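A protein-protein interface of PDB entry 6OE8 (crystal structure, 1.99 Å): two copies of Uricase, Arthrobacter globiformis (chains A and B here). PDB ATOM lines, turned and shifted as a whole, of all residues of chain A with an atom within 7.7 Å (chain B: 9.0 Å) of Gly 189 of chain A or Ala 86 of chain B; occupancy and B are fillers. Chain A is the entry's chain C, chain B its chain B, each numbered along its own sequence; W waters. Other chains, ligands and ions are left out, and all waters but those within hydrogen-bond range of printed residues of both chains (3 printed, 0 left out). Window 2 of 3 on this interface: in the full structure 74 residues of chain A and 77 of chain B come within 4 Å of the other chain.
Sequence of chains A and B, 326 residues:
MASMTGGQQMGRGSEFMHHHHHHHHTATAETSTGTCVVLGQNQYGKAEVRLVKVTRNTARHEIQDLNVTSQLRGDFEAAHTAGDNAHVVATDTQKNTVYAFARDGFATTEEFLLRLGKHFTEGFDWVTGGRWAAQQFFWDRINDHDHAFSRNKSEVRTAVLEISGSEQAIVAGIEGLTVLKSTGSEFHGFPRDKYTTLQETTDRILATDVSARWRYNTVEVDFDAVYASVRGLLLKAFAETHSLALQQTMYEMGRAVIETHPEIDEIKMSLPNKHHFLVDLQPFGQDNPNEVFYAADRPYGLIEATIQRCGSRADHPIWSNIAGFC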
ATOM      1  N   PHE A 187      -2.909  -6.358  27.387  1.00  0.00           N
ATOM      2  CA  PHE A 187      -1.973  -7.381  26.923  1.00  0.00           C
ATOM      3  C   PHE A 187      -0.722  -7.326  27.788  1.00  0.00           C
ATOM      4  O   PHE A 187       0.096  -6.409  27.651  1.00  0.00           O
ATOM      5  CB  PHE A 187      -1.629  -7.240  25.444  1.00  0.00           C
ATOM      6  CG  PHE A 187      -0.770  -8.360  24.924  1.00  0.00           C
ATOM      7  CD1 PHE A 187      -1.212  -9.677  24.988  1.00  0.00           C
ATOM      8  CD2 PHE A 187       0.464  -8.099  24.356  1.00  0.00           C
ATOM      9  CE1 PHE A 187      -0.415 -10.721  24.520  1.00  0.00           C
ATOM     10  CE2 PHE A 187       1.251  -9.126  23.871  1.00  0.00           C
ATOM     11  CZ  PHE A 187       0.812 -10.443  23.956  1.00  0.00           C
ATOM     12  N   HIS A 188      -0.569  -8.312  28.662  1.00  0.00           N
ATOM     13  CA  HIS A 188       0.564  -8.370  29.570  1.00  0.00           C
ATOM     14  C   HIS A 188       0.783  -9.826  29.948  1.00  0.00           C
ATOM     15  O   HIS A 188      -0.048 -10.692  29.662  1.00  0.00           O
ATOM     16  CB  HIS A 188       0.338  -7.483  30.800  1.00  0.00           C
ATOM     17  CG  HIS A 188      -0.910  -7.814  31.561  1.00  0.00           C
ATOM     18  ND1 HIS A 188      -0.997  -8.885  32.422  1.00  0.00           N
ATOM     19  CD2 HIS A 188      -2.125  -7.212  31.586  1.00  0.00           C
ATOM     20  CE1 HIS A 188      -2.210  -8.935  32.942  1.00  0.00           C
ATOM     21  NE2 HIS A 188      -2.915  -7.932  32.451  1.00  0.00           N
ATOM     22  N   GLY A 189       1.939 -10.093  30.555  1.00  0.00           N
ATOM     23  CA  GLY A 189       2.282 -11.439  30.975  1.00  0.00           C
ATOM     24  C   GLY A 189       2.850 -12.329  29.894  1.00  0.00           C
ATOM     25  O   GLY A 189       2.973 -13.539  30.111  1.00  0.00           O
ATOM     26  N   PHE A 190       3.201 -11.778  28.742  1.00  0.00           N
ATOM     27  CA  PHE A 190       3.766 -12.565  27.657  1.00  0.00           C
ATOM     28  C   PHE A 190       5.274 -12.752  27.834  1.00  0.00           C
ATOM     29  O   PHE A 190       5.934 -11.935  28.480  1.00  0.00           O
ATOM     30  CB  PHE A 190       3.469 -11.908  26.308  1.00  0.00           C
ATOM     31  CG  PHE A 190       3.955 -10.483  26.193  1.00  0.00           C
ATOM     32  CD1 PHE A 190       3.128  -9.423  26.533  1.00  0.00           C
ATOM     33  CD2 PHE A 190       5.227 -10.206  25.736  1.00  0.00           C
ATOM     34  CE1 PHE A 190       3.568  -8.107  26.421  1.00  0.00           C
ATOM     35  CE2 PHE A 190       5.674  -8.900  25.625  1.00  0.00           C
ATOM     36  CZ  PHE A 190       4.841  -7.854  25.972  1.00  0.00           C
ATOM     37  N   PRO A 191       5.834 -13.834  27.285  1.00  0.00           N
ATOM     38  CA  PRO A 191       7.265 -14.100  27.478  1.00  0.00           C
ATOM     39  C   PRO A 191       8.113 -13.093  26.720  1.00  0.00           C
ATOM     40  O   PRO A 191       7.672 -12.481  25.741  1.00  0.00           O
ATOM     41  CB  PRO A 191       7.447 -15.513  26.911  1.00  0.00           C
ATOM     42  CG  PRO A 191       6.324 -15.672  25.922  1.00  0.00           C
ATOM     43  CD  PRO A 191       5.170 -14.910  26.523  1.00  0.00           C
ATOM     44  N   ARG A 192       9.334 -12.889  27.212  1.00  0.00           N
ATOM     45  CA  ARG A 192      10.248 -11.924  26.624  1.00  0.00           C
ATOM     46  C   ARG A 192      11.570 -12.587  26.279  1.00  0.00           C
ATOM     47  O   ARG A 192      12.240 -13.139  27.159  1.00  0.00           O
ATOM     48  CB  ARG A 192      10.471 -10.755  27.572  1.00  0.00           C
ATOM     49  CG  ARG A 192       9.185 -10.082  27.911  1.00  0.00           C
ATOM     50  CD  ARG A 192       9.437  -8.917  28.767  1.00  0.00           C
ATOM     51  NE  ARG A 192      10.060  -7.822  28.046  1.00  0.00           N
ATOM     52  CZ  ARG A 192       9.370  -6.895  27.395  1.00  0.00           C
ATOM     53  NH1 ARG A 192       8.046  -6.945  27.390  1.00  0.00           N
ATOM     54  NH2 ARG A 192       9.997  -5.918  26.762  1.00  0.00           N
ATOM     55  N   GLU A 200       4.207  -3.943  28.023  1.00  0.00           N
ATOM     56  CA  GLU A 200       2.933  -4.410  28.549  1.00  0.00           C
ATOM     57  C   GLU A 200       1.981  -3.235  28.736  1.00  0.00           C
ATOM     58  O   GLU A 200       2.405  -2.092  28.917  1.00  0.00           O
ATOM     59  CB  GLU A 200       3.127  -5.147  29.879  1.00  0.00           C
ATOM     60  CG  GLU A 200       3.856  -6.474  29.746  1.00  0.00           C
ATOM     61  CD  GLU A 200       3.930  -7.237  31.056  1.00  0.00           C
ATOM     62  OE1 GLU A 200       3.559  -6.654  32.106  1.00  0.00           O
ATOM     63  OE2 GLU A 200       4.304  -8.439  31.022  1.00  0.00           O
ATOM     64  N   THR A 201       0.681  -3.520  28.681  1.00  0.00           N
ATOM     65  CA  THR A 201      -0.308  -2.474  28.884  1.00  0.00           C
ATOM     66  C   THR A 201      -1.572  -3.052  29.509  1.00  0.00           C
ATOM     67  O   THR A 201      -1.909  -4.230  29.320  1.00  0.00           O
ATOM     68  CB  THR A 201      -0.659  -1.767  27.567  1.00  0.00           C
ATOM     69  OG1 THR A 201      -1.542  -0.675  27.839  1.00  0.00           O
ATOM     70  CG2 THR A 201      -1.368  -2.737  26.618  1.00  0.00           C
ATOM     71  N   LEU A 244      -8.103  -9.762  27.940  1.00  0.00           N
ATOM     72  CA  LEU A 244      -6.700  -9.925  28.290  1.00  0.00           C
ATOM     73  C   LEU A 244      -5.868 -10.390  27.105  1.00  0.00           C
ATOM     74  O   LEU A 244      -4.634 -10.405  27.198  1.00  0.00           O
ATOM     75  CB  LEU A 244      -6.535 -10.930  29.449  1.00  0.00           C
ATOM     76  CG  LEU A 244      -7.260 -10.583  30.749  1.00  0.00           C
ATOM     77  CD1 LEU A 244      -7.058 -11.682  31.800  1.00  0.00           C
ATOM     78  CD2 LEU A 244      -6.843  -9.218  31.281  1.00  0.00           C
ATOM     79  N   TYR B  44      -1.540 -18.312  15.383  1.00  0.00           N
ATOM     80  CA  TYR B  44      -1.571 -16.856  15.514  1.00  0.00           C
ATOM     81  C   TYR B  44      -0.195 -16.271  15.239  1.00  0.00           C
ATOM     82  O   TYR B  44       0.826 -16.926  15.425  1.00  0.00           O
ATOM     83  CB  TYR B  44      -2.018 -16.424  16.915  1.00  0.00           C
ATOM     84  CG  TYR B  44      -0.843 -16.441  17.848  1.00  0.00           C
ATOM     85  CD1 TYR B  44      -0.341 -17.647  18.328  1.00  0.00           C
ATOM     86  CD2 TYR B  44      -0.193 -15.259  18.203  1.00  0.00           C
ATOM     87  CE1 TYR B  44       0.759 -17.681  19.154  1.00  0.00           C
ATOM     88  CE2 TYR B  44       0.908 -15.279  19.024  1.00  0.00           C
ATOM     89  CZ  TYR B  44       1.379 -16.502  19.498  1.00  0.00           C
ATOM     90  OH  TYR B  44       2.477 -16.529  20.320  1.00  0.00           O
ATOM     91  N   ASP B  75       0.613 -25.295  22.088  1.00  0.00           N
ATOM     92  CA  ASP B  75      -0.231 -25.277  23.287  1.00  0.00           C
ATOM     93  C   ASP B  75      -0.599 -23.842  23.635  1.00  0.00           C
ATOM     94  O   ASP B  75       0.115 -23.163  24.377  1.00  0.00           O
ATOM     95  CB  ASP B  75       0.487 -25.949  24.454  1.00  0.00           C
ATOM     96  CG  ASP B  75      -0.393 -26.079  25.690  1.00  0.00           C
ATOM     97  OD1 ASP B  75      -1.579 -25.680  25.653  1.00  0.00           O
ATOM     98  OD2 ASP B  75       0.120 -26.560  26.724  1.00  0.00           O
ATOM     99  N   PHE B  76      -1.743 -23.380  23.121  1.00  0.00           N
ATOM    100  CA  PHE B  76      -2.218 -22.034  23.424  1.00  0.00           C
ATOM    101  C   PHE B  76      -3.581 -22.064  24.110  1.00  0.00           C
ATOM    102  O   PHE B  76      -4.345 -21.101  24.045  1.00  0.00           O
ATOM    103  CB  PHE B  76      -2.229 -21.163  22.165  1.00  0.00           C
ATOM    104  CG  PHE B  76      -0.875 -21.058  21.524  1.00  0.00           C
ATOM    105  CD1 PHE B  76       0.150 -20.388  22.170  1.00  0.00           C
ATOM    106  CD2 PHE B  76      -0.624 -21.620  20.286  1.00  0.00           C
ATOM    107  CE1 PHE B  76       1.404 -20.312  21.612  1.00  0.00           C
ATOM    108  CE2 PHE B  76       0.629 -21.535  19.716  1.00  0.00           C
ATOM    109  CZ  PHE B  76       1.641 -20.889  20.378  1.00  0.00           C
ATOM    110  N   ALA B  78      -4.563 -22.011  27.399  1.00  0.00           N
ATOM    111  CA  ALA B  78      -4.871 -21.084  28.486  1.00  0.00           C
ATOM    112  C   ALA B  78      -4.956 -19.644  27.990  1.00  0.00           C
ATOM    113  O   ALA B  78      -5.682 -18.830  28.571  1.00  0.00           O
ATOM    114  CB  ALA B  78      -3.825 -21.209  29.594  1.00  0.00           C
ATOM    115  N   ALA B  79      -4.241 -19.320  26.917  1.00  0.00           N
ATOM    116  CA  ALA B  79      -4.426 -18.023  26.267  1.00  0.00           C
ATOM    117  C   ALA B  79      -5.880 -17.807  25.872  1.00  0.00           C
ATOM    118  O   ALA B  79      -6.432 -16.722  26.081  1.00  0.00           O
ATOM    119  CB  ALA B  79      -3.518 -17.917  25.045  1.00  0.00           C
ATOM    120  N   HIS B  80      -6.523 -18.838  25.315  1.00  0.00           N
ATOM    121  CA  HIS B  80      -7.903 -18.685  24.873  1.00  0.00           C
ATOM    122  C   HIS B  80      -8.884 -18.792  26.032  1.00  0.00           C
ATOM    123  O   HIS B  80      -9.805 -17.977  26.146  1.00  0.00           O
ATOM    124  CB  HIS B  80      -8.230 -19.721  23.795  1.00  0.00           C
ATOM    125  CG  HIS B  80      -7.492 -19.507  22.508  1.00  0.00           C
ATOM    126  ND1 HIS B  80      -6.211 -19.971  22.303  1.00  0.00           N
ATOM    127  CD2 HIS B  80      -7.863 -18.902  21.353  1.00  0.00           C
ATOM    128  CE1 HIS B  80      -5.817 -19.650  21.083  1.00  0.00           C
ATOM    129  NE2 HIS B  80      -6.805 -19.009  20.482  1.00  0.00           N
ATOM    130  N   ALA B  82      -8.414 -18.562  29.404  1.00  0.00           N
ATOM    131  CA  ALA B  82      -8.205 -17.758  30.600  1.00  0.00           C
ATOM    132  C   ALA B  82      -7.530 -16.410  30.372  1.00  0.00           C
ATOM    133  O   ALA B  82      -7.411 -15.642  31.332  1.00  0.00           O
ATOM    134  CB  ALA B  82      -7.376 -18.548  31.625  1.00  0.00           C
ATOM    135  N   GLY B  83      -7.074 -16.096  29.163  1.00  0.00           N
ATOM    136  CA  GLY B  83      -6.305 -14.878  28.981  1.00  0.00           C
ATOM    137  C   GLY B  83      -4.915 -14.932  29.575  1.00  0.00           C
ATOM    138  O   GLY B  83      -4.306 -13.884  29.808  1.00  0.00           O
ATOM    139  N   ASP B  84      -4.399 -16.132  29.835  1.00  0.00           N
ATOM    140  CA  ASP B  84      -3.034 -16.328  30.317  1.00  0.00           C
ATOM    141  C   ASP B  84      -2.082 -16.288  29.131  1.00  0.00           C
ATOM    142  O   ASP B  84      -2.075 -17.204  28.301  1.00  0.00           O
ATOM    143  CB  ASP B  84      -2.930 -17.661  31.058  1.00  0.00           C
ATOM    144  CG  ASP B  84      -1.572 -17.870  31.707  1.00  0.00           C
ATOM    145  OD1 ASP B  84      -0.696 -16.982  31.589  1.00  0.00           O
ATOM    146  OD2 ASP B  84      -1.380 -18.938  32.325  1.00  0.00           O
ATOM    147  N   ASN B  85      -1.251 -15.245  29.070  1.00  0.00           N
ATOM    148  CA  ASN B  85      -0.381 -15.007  27.926  1.00  0.00           C
ATOM    149  C   ASN B  85       1.023 -15.588  28.098  1.00  0.00           C
ATOM    150  O   ASN B  85       1.912 -15.257  27.314  1.00  0.00           O
ATOM    151  CB  ASN B  85      -0.305 -13.498  27.656  1.00  0.00           C
ATOM    152  CG  ASN B  85      -1.604 -12.954  27.080  1.00  0.00           C
ATOM    153  OD1 ASN B  85      -2.193 -13.558  26.180  1.00  0.00           O
ATOM    154  ND2 ASN B  85      -2.099 -11.867  27.655  1.00  0.00           N
ATOM    155  N   ALA B  86       1.238 -16.469  29.079  1.00  0.00           N
ATOM    156  CA  ALA B  86       2.580 -16.998  29.319  1.00  0.00           C
ATOM    157  C   ALA B  86       3.153 -17.709  28.095  1.00  0.00           C
ATOM    158  O   ALA B  86       4.375 -17.734  27.913  1.00  0.00           O
ATOM    159  CB  ALA B  86       2.565 -17.948  30.530  1.00  0.00           C
ATOM    160  N   HIS B  87       2.309 -18.311  27.253  1.00  0.00           N
ATOM    161  CA  HIS B  87       2.795 -18.989  26.058  1.00  0.00           C
ATOM    162  C   HIS B  87       2.724 -18.124  24.806  1.00  0.00           C
ATOM    163  O   HIS B  87       3.128 -18.581  23.728  1.00  0.00           O
ATOM    164  CB  HIS B  87       2.007 -20.280  25.815  1.00  0.00           C
ATOM    165  CG  HIS B  87       2.270 -21.353  26.827  1.00  0.00           C
ATOM    166  ND1 HIS B  87       1.569 -22.541  26.850  1.00  0.00           N
ATOM    167  CD2 HIS B  87       3.129 -21.404  27.873  1.00  0.00           C
ATOM    168  CE1 HIS B  87       2.004 -23.289  27.850  1.00  0.00           C
ATOM    169  NE2 HIS B  87       2.944 -22.620  28.492  1.00  0.00           N
ATOM    170  N   VAL B  88       2.217 -16.897  24.910  1.00  0.00           N
ATOM    171  CA  VAL B  88       1.900 -16.096  23.725  1.00  0.00           C
ATOM    172  C   VAL B  88       3.141 -15.268  23.413  1.00  0.00           C
ATOM    173  O   VAL B  88       3.296 -14.139  23.876  1.00  0.00           O
ATOM    174  CB  VAL B  88       0.658 -15.234  23.928  1.00  0.00           C
ATOM    175  CG1 VAL B  88       0.345 -14.451  22.649  1.00  0.00           C
ATOM    176  CG2 VAL B  88      -0.526 -16.098  24.336  1.00  0.00           C
ATOM    177  N   VAL B  89       4.049 -15.851  22.633  1.00  0.00           N
ATOM    178  CA  VAL B  89       5.111 -15.070  22.010  1.00  0.00           C
ATOM    179  C   VAL B  89       4.470 -13.952  21.200  1.00  0.00           C
ATOM    180  O   VAL B  89       3.674 -14.214  20.288  1.00  0.00           O
ATOM    181  CB  VAL B  89       5.996 -15.967  21.135  1.00  0.00           C
ATOM    182  CG1 VAL B  89       7.058 -15.126  20.399  1.00  0.00           C
ATOM    183  CG2 VAL B  89       6.637 -17.054  21.979  1.00  0.00           C
ATOM    184  N   ALA B  90       4.800 -12.704  21.538  1.00  0.00           N
ATOM    185  CA  ALA B  90       4.075 -11.559  20.992  1.00  0.00           C
ATOM    186  C   ALA B  90       4.168 -11.526  19.471  1.00  0.00           C
ATOM    187  O   ALA B  90       5.203 -11.862  18.888  1.00  0.00           O
ATOM    188  CB  ALA B  90       4.626 -10.251  21.572  1.00  0.00           C
ATOM    189  N   PHE B 124      10.940 -22.496  21.731  1.00  0.00           N
ATOM    190  CA  PHE B 124       9.864 -22.470  22.709  1.00  0.00           C
ATOM    191  C   PHE B 124       9.282 -23.866  22.854  1.00  0.00           C
ATOM    192  O   PHE B 124       8.880 -24.481  21.861  1.00  0.00           O
ATOM    193  CB  PHE B 124       8.786 -21.462  22.298  1.00  0.00           C
ATOM    194  CG  PHE B 124       9.292 -20.049  22.234  1.00  0.00           C
ATOM    195  CD1 PHE B 124       9.409 -19.286  23.383  1.00  0.00           C
ATOM    196  CD2 PHE B 124       9.708 -19.506  21.033  1.00  0.00           C
ATOM    197  CE1 PHE B 124       9.891 -17.985  23.331  1.00  0.00           C
ATOM    198  CE2 PHE B 124      10.197 -18.205  20.973  1.00  0.00           C
ATOM    199  CZ  PHE B 124      10.288 -17.450  22.128  1.00  0.00           C
ATOM    200  N   TRP B 126       6.475 -25.034  24.188  1.00  0.00           N
ATOM    201  CA  TRP B 126       5.061 -25.214  23.883  1.00  0.00           C
ATOM    202  C   TRP B 126       4.714 -24.928  22.425  1.00  0.00           C
ATOM    203  O   TRP B 126       3.566 -25.160  22.029  1.00  0.00           O
ATOM    204  CB  TRP B 126       4.226 -24.295  24.777  1.00  0.00           C
ATOM    205  CG  TRP B 126       4.623 -22.861  24.607  1.00  0.00           C
ATOM    206  CD1 TRP B 126       4.133 -21.981  23.687  1.00  0.00           C
ATOM    207  CD2 TRP B 126       5.616 -22.148  25.357  1.00  0.00           C
ATOM    208  NE1 TRP B 126       4.749 -20.762  23.825  1.00  0.00           N
ATOM    209  CE2 TRP B 126       5.665 -20.838  24.842  1.00  0.00           C
ATOM    210  CE3 TRP B 126       6.465 -22.490  26.416  1.00  0.00           C
ATOM    211  CZ2 TRP B 126       6.522 -19.869  25.347  1.00  0.00           C
ATOM    212  CZ3 TRP B 126       7.316 -21.519  26.919  1.00  0.00           C
ATOM    213  CH2 TRP B 126       7.339 -20.226  26.381  1.00  0.00           C
ATOM    214  N   VAL B 127       5.661 -24.447  21.619  1.00  0.00           N
ATOM    215  CA  VAL B 127       5.436 -24.244  20.189  1.00  0.00           C
ATOM    216  C   VAL B 127       5.840 -25.513  19.457  1.00  0.00           C
ATOM    217  O   VAL B 127       7.014 -25.900  19.464  1.00  0.00           O
ATOM    218  CB  VAL B 127       6.219 -23.032  19.658  1.00  0.00           C
ATOM    219  CG1 VAL B 127       6.084 -22.935  18.134  1.00  0.00           C
ATOM    220  CG2 VAL B 127       5.722 -21.758  20.307  1.00  0.00           C
HETATM  221  O   HOH W   1       7.270 -12.321  23.148  1.00  0.00           O
HETATM  222  O   HOH W   2      -3.174  -9.487  29.283  1.00  0.00           O
HETATM  223  O   HOH W   3      -1.004 -13.041  31.056  1.00  0.00           O
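Of the 9 printed residues of chain A, 6 touch a printed residue of chain B.
Among the printed residues, 11 pairs touch across the chains.
Among the printed residues, no Asp or Glu carboxylate lies within 4 Å of a Lys or Arg side-chain nitrogen of the other chain.
Phe 187 of chain A touches Asn 85 of chain B (CD1 to ND2, 3.6 Å).
O of Gly 189 of chain A touches N of Ala 86 of chain B, at 3.6 Å.
CA of Phe 190 of chain A touches O of Asn 85 of chain B (3.3 Å).
CB of Phe 190 of chain A touches O of Val 88 of chain B, 3.3 Å away.
CD of Pro 191 of chain A touches O of Asn 85 of chain B (3.4 Å).
Pro 191 of chain A touches Ala 86 of chain B.
Pro 191 of chain A touches Val 88 of chain B (CD to O, 3.3 Å).
Leu 244 of chain A touches Gly 83 of chain B (CB to O, 3.7 Å).
The backbone carbonyl oxygen (O) of His 188 of chain A sits at hydrogen-bond distance from the side-chain amide nitrogen (ND2) of Asn 85 of chain B (3.1 Å).
O of Leu 244 of chain A is in hydrogen-bond range of ND2 of Asn 85 of chain B (3.0 Å).
The backbone carbonyl oxygen (O) of Asn 85 of chain B sits close to the backbone carbonyl oxygen (O) of Gly 189 of chain A (3.4 Å).
Water W1 bridges the backbone carbonyl oxygen (O) of Pro 191 of chain A and the backbone NH (N) of Ala 90 of chain B.
Water W2 lies within hydrogen-bond range of the backbone carbonyl oxygen of Leu 244 of chain A (2.7 Å), the backbone NH of His 188 of chain A (2.9 Å) and the side-chain amide nitrogen of Asn 85 of chain B (3.1 Å).
Water W3 lies within hydrogen-bond range of the backbone carbonyl oxygen (O) of His 188 of chain A and the backbone NH (N) of Asn 85 of chain B.
No position is printed for both chains.
The side-chain carboxylate (OD1) of Asp 84 of chain B sits at hydrogen-bond distance from the backbone NH (N) of Ala 86 of chain B (3.2 Å).
The backbone carbonyl oxygen of Thr 201 of chain A is in hydrogen-bond range of the backbone NH of Phe 187 of chain A (3.0 Å).
The backbone carbonyl oxygen (O) of Ala 78 of chain B lies within hydrogen-bond range of the backbone NH (N) of Gly 83 of chain B, 3.1 Å away.
N of Gly 189 of chain A sits at hydrogen-bond distance from OE2 of Glu 200 of chain A (2.9 Å).
Printed residues of chain B within 4 Å of His 188 of chain A: Asn 85.
Gly 189 of chain A touches just these residues of chain B: Asn 85 and Ala 86.
Of the printed residues of chain B, Pro 191 of chain A touches Asn 85, Ala 86 and Val 88.
Printed residues of chain B within 4 Å of Leu 244 of chain A: Gly 83 (3.7 Å) and Asn 85 (3.0 Å).
Of chain A, only Gly 189 (3.6 Å) and Pro 191 (3.2 Å) come within 4 Å of Ala 86 of chain B.
Ala 90 of chain B touches none of the printed residues of chain A.
The nearest residue of chain B that does not touch Gly 189 of chain A is Asp 84 of chain B (5.2 Å).
The nearest residue of chain A that does not touch Ala 86 of chain B is Phe 190 of chain A (4.9 Å).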
